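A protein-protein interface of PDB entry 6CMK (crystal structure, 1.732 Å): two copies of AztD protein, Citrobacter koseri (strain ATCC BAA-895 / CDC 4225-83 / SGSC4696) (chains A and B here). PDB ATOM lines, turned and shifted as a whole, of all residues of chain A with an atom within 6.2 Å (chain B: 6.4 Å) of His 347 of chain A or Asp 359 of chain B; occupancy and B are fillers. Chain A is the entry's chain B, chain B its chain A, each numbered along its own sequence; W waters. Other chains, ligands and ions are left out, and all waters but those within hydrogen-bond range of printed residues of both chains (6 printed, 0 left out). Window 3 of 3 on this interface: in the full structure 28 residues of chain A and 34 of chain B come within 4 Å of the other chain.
OD2 of Asp 32 of chain B lies within hydrogen-bond range of NE1 of Trp 348 of chain A (2.6 Å).
The side-chain hydroxyl (OG) of Ser 401 of chain B sits at hydrogen-bond distance from the backbone NH (N) of Trp 348 of chain A, 3.1 Å away.
Water W2 bridges OD2 of Asp 359 of chain B and NE2 of His 347 of chain A.
Water W4 lies within hydrogen-bond range of the side-chain carboxylate of Asp 32 of chain B (2.6 Å), the side-chain amide oxygen of Asn 349 of chain A (2.7 Å) and the side-chain hydroxyl of Ser 401 of chain B (2.7 Å).
Water W1 lies within hydrogen-bond range of the backbone carbonyl oxygen (O) of Gly 346 of chain A (2.8 Å), the indole nitrogen (NE1) of Trp 36 of chain B (2.8 Å) and the side-chain carboxylate (OD1) of Asp 359 of chain B (3.1 Å).
Water W3 lies within hydrogen-bond range of O of Val 308 of chain B (2.8 Å) and N of Ser 343 of chain A (3.1 Å).
Water W6 bridges the side-chain hydroxyl (OG1) of Thr 34 of chain B (3.0 Å) and a ring nitrogen (NE2) of His 347 of chain A (3.5 Å).
Water W5 lies within hydrogen-bond range of OD1 of Asp 32 of chain B (3.0 Å) and ND2 of Asn 349 of chain A (3.2 Å).
The backbone carbonyl oxygen of Trp 348 of chain A lies within hydrogen-bond range of the guanidinium group of Arg 352 of chain A (3.2 Å).
The guanidinium group (NH2) of Arg 352 of chain A is in hydrogen-bond range of the backbone carbonyl oxygen (O) of His 347 of chain A (3.0 Å).
O of Asp 359 of chain B is in hydrogen-bond range of NH2 of Arg 309 of chain B (2.8 Å).
The side-chain hydroxyl (OG) of Ser 343 of chain A sits at hydrogen-bond distance from the backbone NH (N) of Asp 345 of chain A (3.0 Å).
The side-chain carboxylate of Asp 306 of chain B lies within hydrogen-bond range of the backbone NH of Val 308 of chain B (2.9 Å).
O of Ser 343 of chain A sits at hydrogen-bond distance from NE of Arg 352 of chain A (2.9 Å).
Of the printed residues of chain B, Gly 346 of chain A touches Trp 36 (3.8 Å), Val 308 (3.9 Å), Gly 400 (3.4 Å) and Ser 401 (3.7 Å).
His 347 of chain A touches three residues of chain B.
Printed residues of chain A within 4 Å of Trp 36 of chain B: Gly 346 (3.8 Å).
Of the printed residues of chain A, Val 308 of chain B touches Ser 343 (3.5 Å) and Gly 346 (3.9 Å).
Asn 360 of chain B touches none of the printed residues of chain A.
Of the printed residues of chain A, Ser 401 of chain B touches Gly 346 (3.7 Å), His 347 (3.2 Å) and Trp 348 (3.1 Å).
Of the printed residues of chain A, Gly 402 of chain B touches Trp 348 (3.4 Å).
The nearest residue of chain B that does not touch His 347 of chain A is Asn 360 of chain B (4.4 Å).
The nearest residue of chain A that does not touch Asp 359 of chain B is Gly 346 of chain A (4.8 Å).
Of the 17 printed residues of chain B, 8 touch a printed residue of chain A.
Printed residues of chain B that touch a printed residue of chain A: Asp 32, Thr 34, Trp 36, Val 308, Asp 359, Gly 400, Ser 401 and Gly 402.
Of the 9 printed residues of chain A, 5 touch a printed residue of chain B.
Hydrophobic or aromatic side chains of chain A that line the printed part of chain B: His 347 and Trp 348.
Along chain A the printed residues that touch a printed residue of chain B span positions 343 to 349.
Among the printed residues, 12 pairs touch across the chains.
Among the printed residues, pairs that only touch across the chains: Ser 343 of chain A with Val 308 of chain B, Gly 346 of chain A with Trp 36 of chain B, Gly 346 of chain A with Val 308 of chain B, Gly 346 of chain A with Gly 400 of chain B, Gly 346 of chain A with Ser 401 of chain B, His 347 of chain A with Thr 34 of chain B, His 347 of chain A with Asp 359 of chain B, His 347 of chain A with Ser 401 of chain B, Trp 348 of chain A with Gly 402 of chain B and Asn 349 of chain A with Asp 32 of chain B.
No position is printed for both chains.
Of the 12 pairs that touch across the chains among the printed residues, none has its exchanged pair printed and touching as well.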
ATOM      1  N   SER A 343     -18.166  25.696  -2.377  1.00  0.00           N
ATOM      2  CA  SER A 343     -17.147  25.442  -3.384  1.00  0.00           C
ATOM      3  C   SER A 343     -17.680  25.687  -4.789  1.00  0.00           C
ATOM      4  O   SER A 343     -18.827  25.369  -5.109  1.00  0.00           O
ATOM      5  CB  SER A 343     -16.655  23.998  -3.296  1.00  0.00           C
ATOM      6  OG  SER A 343     -15.707  23.765  -4.312  1.00  0.00           O
ATOM      7  N   MET A 344     -16.810  26.205  -5.652  1.00  0.00           N
ATOM      8  CA  MET A 344     -17.128  26.362  -7.062  1.00  0.00           C
ATOM      9  C   MET A 344     -16.940  25.076  -7.857  1.00  0.00           C
ATOM     10  O   MET A 344     -17.238  25.050  -9.058  1.00  0.00           O
ATOM     11  CB  MET A 344     -16.293  27.508  -7.656  1.00  0.00           C
ATOM     12  CG  MET A 344     -16.781  28.875  -7.196  1.00  0.00           C
ATOM     13  SD  MET A 344     -18.451  29.207  -7.781  1.00  0.00           S
ATOM     14  CE  MET A 344     -18.135  29.538  -9.502  1.00  0.00           C
ATOM     15  N   ASP A 345     -16.521  23.991  -7.210  1.00  0.00           N
ATOM     16  CA  ASP A 345     -16.573  22.694  -7.847  1.00  0.00           C
ATOM     17  C   ASP A 345     -17.920  22.033  -7.567  1.00  0.00           C
ATOM     18  O   ASP A 345     -18.658  22.424  -6.658  1.00  0.00           O
ATOM     19  CB  ASP A 345     -15.430  21.822  -7.352  1.00  0.00           C
ATOM     20  CG  ASP A 345     -14.120  22.198  -7.988  1.00  0.00           C
ATOM     21  OD1 ASP A 345     -14.078  22.203  -9.236  1.00  0.00           O
ATOM     22  OD2 ASP A 345     -13.161  22.523  -7.258  1.00  0.00           O
ATOM     23  N   GLY A 346     -18.231  21.018  -8.363  1.00  0.00           N
ATOM     24  CA  GLY A 346     -19.523  20.360  -8.289  1.00  0.00           C
ATOM     25  C   GLY A 346     -20.264  20.544  -9.589  1.00  0.00           C
ATOM     26  O   GLY A 346     -19.754  20.189 -10.651  1.00  0.00           O
ATOM     27  N   HIS A 347     -21.468  21.106  -9.522  1.00  0.00           N
ATOM     28  CA  HIS A 347     -22.215  21.500 -10.708  1.00  0.00           C
ATOM     29  C   HIS A 347     -22.187  23.014 -10.852  1.00  0.00           C
ATOM     30  O   HIS A 347     -22.144  23.744  -9.862  1.00  0.00           O
ATOM     31  CB  HIS A 347     -23.677  21.040 -10.638  1.00  0.00           C
ATOM     32  CG  HIS A 347     -23.849  19.583 -10.350  1.00  0.00           C
ATOM     33  ND1 HIS A 347     -24.168  19.107  -9.097  1.00  0.00           N
ATOM     34  CD2 HIS A 347     -23.768  18.497 -11.158  1.00  0.00           C
ATOM     35  CE1 HIS A 347     -24.273  17.790  -9.143  1.00  0.00           C
ATOM     36  NE2 HIS A 347     -24.034  17.395 -10.382  1.00  0.00           N
ATOM     37  N   TRP A 348     -22.231  23.481 -12.098  1.00  0.00           N
ATOM     38  CA  TRP A 348     -22.258  24.921 -12.319  1.00  0.00           C
ATOM     39  C   TRP A 348     -23.501  25.535 -11.700  1.00  0.00           C
ATOM     40  O   TRP A 348     -23.456  26.674 -11.223  1.00  0.00           O
ATOM     41  CB  TRP A 348     -22.206  25.239 -13.810  1.00  0.00           C
ATOM     42  CG  TRP A 348     -23.487  24.970 -14.545  1.00  0.00           C
ATOM     43  CD1 TRP A 348     -23.843  23.817 -15.176  1.00  0.00           C
ATOM     44  CD2 TRP A 348     -24.582  25.879 -14.731  1.00  0.00           C
ATOM     45  NE1 TRP A 348     -25.086  23.949 -15.744  1.00  0.00           N
ATOM     46  CE2 TRP A 348     -25.560  25.205 -15.485  1.00  0.00           C
ATOM     47  CE3 TRP A 348     -24.825  27.197 -14.333  1.00  0.00           C
ATOM     48  CZ2 TRP A 348     -26.770  25.802 -15.847  1.00  0.00           C
ATOM     49  CZ3 TRP A 348     -26.027  27.789 -14.694  1.00  0.00           C
ATOM     50  CH2 TRP A 348     -26.981  27.093 -15.442  1.00  0.00           C
ATOM     51  N   ASN A 349     -24.600  24.783 -11.678  1.00  0.00           N
ATOM     52  CA  ASN A 349     -25.880  25.265 -11.185  1.00  0.00           C
ATOM     53  C   ASN A 349     -26.248  24.669  -9.829  1.00  0.00           C
ATOM     54  O   ASN A 349     -27.432  24.589  -9.486  1.00  0.00           O
ATOM     55  CB  ASN A 349     -26.976  25.003 -12.218  1.00  0.00           C
ATOM     56  CG  ASN A 349     -27.073  23.545 -12.652  1.00  0.00           C
ATOM     57  OD1 ASN A 349     -26.167  22.739 -12.439  1.00  0.00           O
ATOM     58  ND2 ASN A 349     -28.192  23.205 -13.296  1.00  0.00           N
ATOM     59  N   ASP A 350     -25.254  24.273  -9.032  1.00  0.00           N
ATOM     60  CA  ASP A 350     -25.503  24.138  -7.602  1.00  0.00           C
ATOM     61  C   ASP A 350     -25.881  25.511  -7.044  1.00  0.00           C
ATOM     62  O   ASP A 350     -25.342  26.533  -7.488  1.00  0.00           O
ATOM     63  CB  ASP A 350     -24.269  23.604  -6.855  1.00  0.00           C
ATOM     64  CG  ASP A 350     -23.982  22.134  -7.134  1.00  0.00           C
ATOM     65  OD1 ASP A 350     -24.930  21.374  -7.432  1.00  0.00           O
ATOM     66  OD2 ASP A 350     -22.801  21.729  -7.021  1.00  0.00           O
ATOM     67  N   ARG A 352     -25.763  28.790  -4.978  1.00  0.00           N
ATOM     68  CA  ARG A 352     -24.690  29.509  -4.313  1.00  0.00           C
ATOM     69  C   ARG A 352     -25.101  30.951  -4.072  1.00  0.00           C
ATOM     70  O   ARG A 352     -26.038  31.454  -4.709  1.00  0.00           O
ATOM     71  CB  ARG A 352     -23.391  29.486  -5.135  1.00  0.00           C
ATOM     72  CG  ARG A 352     -22.857  28.090  -5.430  1.00  0.00           C
ATOM     73  CD  ARG A 352     -21.487  28.158  -6.089  1.00  0.00           C
ATOM     74  NE  ARG A 352     -20.927  26.839  -6.376  1.00  0.00           N
ATOM     75  CZ  ARG A 352     -21.179  26.129  -7.473  1.00  0.00           C
ATOM     76  NH1 ARG A 352     -22.006  26.592  -8.399  1.00  0.00           N
ATOM     77  NH2 ARG A 352     -20.598  24.945  -7.644  1.00  0.00           N
ATOM     78  N   ASP B  32     -27.435  20.434 -20.718  1.00  0.00           N
ATOM     79  CA  ASP B  32     -26.632  20.563 -19.507  1.00  0.00           C
ATOM     80  C   ASP B  32     -25.879  19.255 -19.301  1.00  0.00           C
ATOM     81  O   ASP B  32     -26.502  18.200 -19.149  1.00  0.00           O
ATOM     82  CB  ASP B  32     -27.538  20.873 -18.314  1.00  0.00           C
ATOM     83  CG  ASP B  32     -26.821  21.587 -17.206  1.00  0.00           C
ATOM     84  OD1 ASP B  32     -25.991  20.949 -16.527  1.00  0.00           O
ATOM     85  OD2 ASP B  32     -27.094  22.791 -17.015  1.00  0.00           O
ATOM     86  N   THR B  34     -22.817  16.920 -17.469  1.00  0.00           N
ATOM     87  CA  THR B  34     -21.921  16.613 -16.362  1.00  0.00           C
ATOM     88  C   THR B  34     -20.870  15.638 -16.864  1.00  0.00           C
ATOM     89  O   THR B  34     -21.201  14.641 -17.512  1.00  0.00           O
ATOM     90  CB  THR B  34     -22.685  15.993 -15.185  1.00  0.00           C
ATOM     91  OG1 THR B  34     -23.639  16.931 -14.669  1.00  0.00           O
ATOM     92  CG2 THR B  34     -21.733  15.591 -14.068  1.00  0.00           C
ATOM     93  N   TRP B  36     -16.988  13.855 -15.617  1.00  0.00           N
ATOM     94  CA  TRP B  36     -15.836  13.694 -14.742  1.00  0.00           C
ATOM     95  C   TRP B  36     -15.022  12.496 -15.212  1.00  0.00           C
ATOM     96  O   TRP B  36     -15.584  11.488 -15.650  1.00  0.00           O
ATOM     97  CB  TRP B  36     -16.239  13.471 -13.286  1.00  0.00           C
ATOM     98  CG  TRP B  36     -16.924  14.636 -12.602  1.00  0.00           C
ATOM     99  CD1 TRP B  36     -18.209  15.049 -12.785  1.00  0.00           C
ATOM    100  CD2 TRP B  36     -16.367  15.489 -11.601  1.00  0.00           C
ATOM    101  NE1 TRP B  36     -18.492  16.115 -11.965  1.00  0.00           N
ATOM    102  CE2 TRP B  36     -17.373  16.409 -11.230  1.00  0.00           C
ATOM    103  CE3 TRP B  36     -15.120  15.576 -10.988  1.00  0.00           C
ATOM    104  CZ2 TRP B  36     -17.164  17.388 -10.274  1.00  0.00           C
ATOM    105  CZ3 TRP B  36     -14.920  16.554 -10.036  1.00  0.00           C
ATOM    106  CH2 TRP B  36     -15.937  17.446  -9.693  1.00  0.00           C
ATOM    107  N   LEU B  54     -18.263   8.610 -13.917  1.00  0.00           N
ATOM    108  CA  LEU B  54     -19.678   8.493 -13.582  1.00  0.00           C
ATOM    109  C   LEU B  54     -20.224   7.087 -13.833  1.00  0.00           C
ATOM    110  O   LEU B  54     -21.176   6.674 -13.161  1.00  0.00           O
ATOM    111  CB  LEU B  54     -20.469   9.552 -14.358  1.00  0.00           C
ATOM    112  CG  LEU B  54     -19.906  10.982 -14.250  1.00  0.00           C
ATOM    113  CD1 LEU B  54     -20.819  11.996 -14.925  1.00  0.00           C
ATOM    114  CD2 LEU B  54     -19.649  11.404 -12.803  1.00  0.00           C
ATOM    115  N   ASP B 306     -11.813  17.000  -0.097  1.00  0.00           N
ATOM    116  CA  ASP B 306     -13.005  16.928  -0.926  1.00  0.00           C
ATOM    117  C   ASP B 306     -13.176  18.289  -1.588  1.00  0.00           C
ATOM    118  O   ASP B 306     -13.405  19.281  -0.880  1.00  0.00           O
ATOM    119  CB  ASP B 306     -14.230  16.570  -0.101  1.00  0.00           C
ATOM    120  CG  ASP B 306     -15.443  16.220  -0.964  1.00  0.00           C
ATOM    121  OD1 ASP B 306     -15.704  16.923  -1.969  1.00  0.00           O
ATOM    122  OD2 ASP B 306     -16.151  15.248  -0.622  1.00  0.00           O
ATOM    123  N   VAL B 308     -15.522  19.339  -3.608  1.00  0.00           N
ATOM    124  CA  VAL B 308     -16.926  19.704  -3.760  1.00  0.00           C
ATOM    125  C   VAL B 308     -17.559  20.043  -2.415  1.00  0.00           C
ATOM    126  O   VAL B 308     -18.270  21.044  -2.286  1.00  0.00           O
ATOM    127  CB  VAL B 308     -17.676  18.555  -4.473  1.00  0.00           C
ATOM    128  CG1 VAL B 308     -19.168  18.862  -4.577  1.00  0.00           C
ATOM    129  CG2 VAL B 308     -17.100  18.304  -5.851  1.00  0.00           C
ATOM    130  N   ARG B 309     -17.339  19.201  -1.400  1.00  0.00           N
ATOM    131  CA  ARG B 309     -17.829  19.441  -0.044  1.00  0.00           C
ATOM    132  C   ARG B 309     -16.649  19.958   0.776  1.00  0.00           C
ATOM    133  O   ARG B 309     -15.886  19.198   1.369  1.00  0.00           O
ATOM    134  CB  ARG B 309     -18.445  18.178   0.546  1.00  0.00           C
ATOM    135  CG  ARG B 309     -19.680  17.697  -0.207  1.00  0.00           C
ATOM    136  CD  ARG B 309     -19.783  16.176  -0.216  1.00  0.00           C
ATOM    137  NE  ARG B 309     -18.794  15.640  -1.150  1.00  0.00           N
ATOM    138  CZ  ARG B 309     -19.002  15.475  -2.454  1.00  0.00           C
ATOM    139  NH1 ARG B 309     -20.195  15.749  -2.996  1.00  0.00           N
ATOM    140  NH2 ARG B 309     -18.024  15.012  -3.214  1.00  0.00           N
ATOM    141  N   VAL B 357     -11.570  12.126  -5.566  1.00  0.00           N
ATOM    142  CA  VAL B 357     -12.965  12.542  -5.434  1.00  0.00           C
ATOM    143  C   VAL B 357     -13.438  13.109  -6.767  1.00  0.00           C
ATOM    144  O   VAL B 357     -12.754  13.943  -7.363  1.00  0.00           O
ATOM    145  CB  VAL B 357     -13.154  13.595  -4.325  1.00  0.00           C
ATOM    146  CG1 VAL B 357     -14.642  13.913  -4.155  1.00  0.00           C
ATOM    147  CG2 VAL B 357     -12.566  13.117  -3.008  1.00  0.00           C
ATOM    148  N   ALA B 358     -14.614  12.669  -7.220  1.00  0.00           N
ATOM    149  CA  ALA B 358     -15.242  13.206  -8.420  1.00  0.00           C
ATOM    150  C   ALA B 358     -16.739  13.299  -8.180  1.00  0.00           C
ATOM    151  O   ALA B 358     -17.365  12.314  -7.779  1.00  0.00           O
ATOM    152  CB  ALA B 358     -14.972  12.336  -9.653  1.00  0.00           C
ATOM    153  N   ASP B 359     -17.304  14.483  -8.430  1.00  0.00           N
ATOM    154  CA  ASP B 359     -18.746  14.733  -8.309  1.00  0.00           C
ATOM    155  C   ASP B 359     -19.162  14.344  -6.892  1.00  0.00           C
ATOM    156  O   ASP B 359     -18.608  14.895  -5.928  1.00  0.00           O
ATOM    157  CB  ASP B 359     -19.477  13.998  -9.437  1.00  0.00           C
ATOM    158  CG  ASP B 359     -20.847  14.576  -9.722  1.00  0.00           C
ATOM    159  OD1 ASP B 359     -21.102  15.735  -9.330  1.00  0.00           O
ATOM    160  OD2 ASP B 359     -21.674  13.871 -10.333  1.00  0.00           O
ATOM    161  N   ASN B 360     -20.095  13.419  -6.715  1.00  0.00           N
ATOM    162  CA  ASN B 360     -20.554  13.038  -5.384  1.00  0.00           C
ATOM    163  C   ASN B 360     -20.056  11.652  -4.993  1.00  0.00           C
ATOM    164  O   ASN B 360     -20.708  10.939  -4.227  1.00  0.00           O
ATOM    165  CB  ASN B 360     -22.075  13.114  -5.330  1.00  0.00           C
ATOM    166  CG  ASN B 360     -22.586  14.521  -5.594  1.00  0.00           C
ATOM    167  OD1 ASN B 360     -21.900  15.511  -5.301  1.00  0.00           O
ATOM    168  ND2 ASN B 360     -23.783  14.621  -6.163  1.00  0.00           N
ATOM    169  N   LYS B 361     -18.892  11.268  -5.510  1.00  0.00           N
ATOM    170  CA  LYS B 361     -18.335   9.945  -5.293  1.00  0.00           C
ATOM    171  C   LYS B 361     -16.881  10.045  -4.855  1.00  0.00           C
ATOM    172  O   LYS B 361     -16.146  10.966  -5.240  1.00  0.00           O
ATOM    173  CB  LYS B 361     -18.425   9.089  -6.562  1.00  0.00           C
ATOM    174  CG  LYS B 361     -19.836   8.713  -6.938  1.00  0.00           C
ATOM    175  CD  LYS B 361     -19.878   8.075  -8.310  1.00  0.00           C
ATOM    176  CE  LYS B 361     -21.200   7.368  -8.557  1.00  0.00           C
ATOM    177  NZ  LYS B 361     -21.152   6.513  -9.775  1.00  0.00           N
ATOM    178  N   TYR B 363     -13.330   7.648  -4.689  1.00  0.00           N
ATOM    179  CA  TYR B 363     -12.701   6.551  -5.418  1.00  0.00           C
ATOM    180  C   TYR B 363     -11.436   6.132  -4.688  1.00  0.00           C
ATOM    181  O   TYR B 363     -10.590   6.972  -4.371  1.00  0.00           O
ATOM    182  CB  TYR B 363     -12.365   6.957  -6.858  1.00  0.00           C
ATOM    183  CG  TYR B 363     -13.571   7.376  -7.637  1.00  0.00           C
ATOM    184  CD1 TYR B 363     -14.117   8.643  -7.469  1.00  0.00           C
ATOM    185  CD2 TYR B 363     -14.203   6.494  -8.504  1.00  0.00           C
ATOM    186  CE1 TYR B 363     -15.247   9.023  -8.151  1.00  0.00           C
ATOM    187  CE2 TYR B 363     -15.338   6.878  -9.201  1.00  0.00           C
ATOM    188  CZ  TYR B 363     -15.842   8.150  -9.017  1.00  0.00           C
ATOM    189  OH  TYR B 363     -16.979   8.551  -9.698  1.00  0.00           O
ATOM    190  N   ALA B 377     -20.330   9.891  -1.494  1.00  0.00           N
ATOM    191  CA  ALA B 377     -19.580  10.744  -0.577  1.00  0.00           C
ATOM    192  C   ALA B 377     -20.370  11.074   0.682  1.00  0.00           C
ATOM    193  O   ALA B 377     -19.787  11.165   1.769  1.00  0.00           O
ATOM    194  CB  ALA B 377     -19.157  12.037  -1.270  1.00  0.00           C
ATOM    195  N   GLY B 400     -16.746  18.408 -13.767  1.00  0.00           N
ATOM    196  CA  GLY B 400     -17.777  19.335 -13.309  1.00  0.00           C
ATOM    197  C   GLY B 400     -18.969  19.273 -14.256  1.00  0.00           C
ATOM    198  O   GLY B 400     -19.219  18.252 -14.882  1.00  0.00           O
ATOM    199  N   SER B 401     -19.680  20.390 -14.380  1.00  0.00           N
ATOM    200  CA  SER B 401     -20.787  20.412 -15.329  1.00  0.00           C
ATOM    201  C   SER B 401     -20.913  21.804 -15.932  1.00  0.00           C
ATOM    202  O   SER B 401     -20.422  22.791 -15.386  1.00  0.00           O
ATOM    203  CB  SER B 401     -22.106  19.978 -14.672  1.00  0.00           C
ATOM    204  OG  SER B 401     -22.660  21.010 -13.874  1.00  0.00           O
ATOM    205  N   GLY B 402     -21.557  21.863 -17.089  1.00  0.00           N
ATOM    206  CA  GLY B 402     -21.742  23.140 -17.747  1.00  0.00           C
ATOM    207  C   GLY B 402     -22.772  23.021 -18.842  1.00  0.00           C
ATOM    208  O   GLY B 402     -23.298  21.944 -19.124  1.00  0.00           O
HETATM  209  O   HOH W   1     -20.753  17.762 -11.604  1.00  0.00           O
HETATM  210  O   HOH W   2     -24.000  14.716 -10.686  1.00  0.00           O
HETATM  211  O   HOH W   3     -18.541  23.242  -0.512  1.00  0.00           O
HETATM  212  O   HOH W   4     -25.350  20.765 -14.023  1.00  0.00           O
HETATM  213  O   HOH W   5     -28.695  20.752 -15.290  1.00  0.00           O
HETATM  214  O   HOH W   6     -25.381  15.347 -12.878  1.00  0.00           O
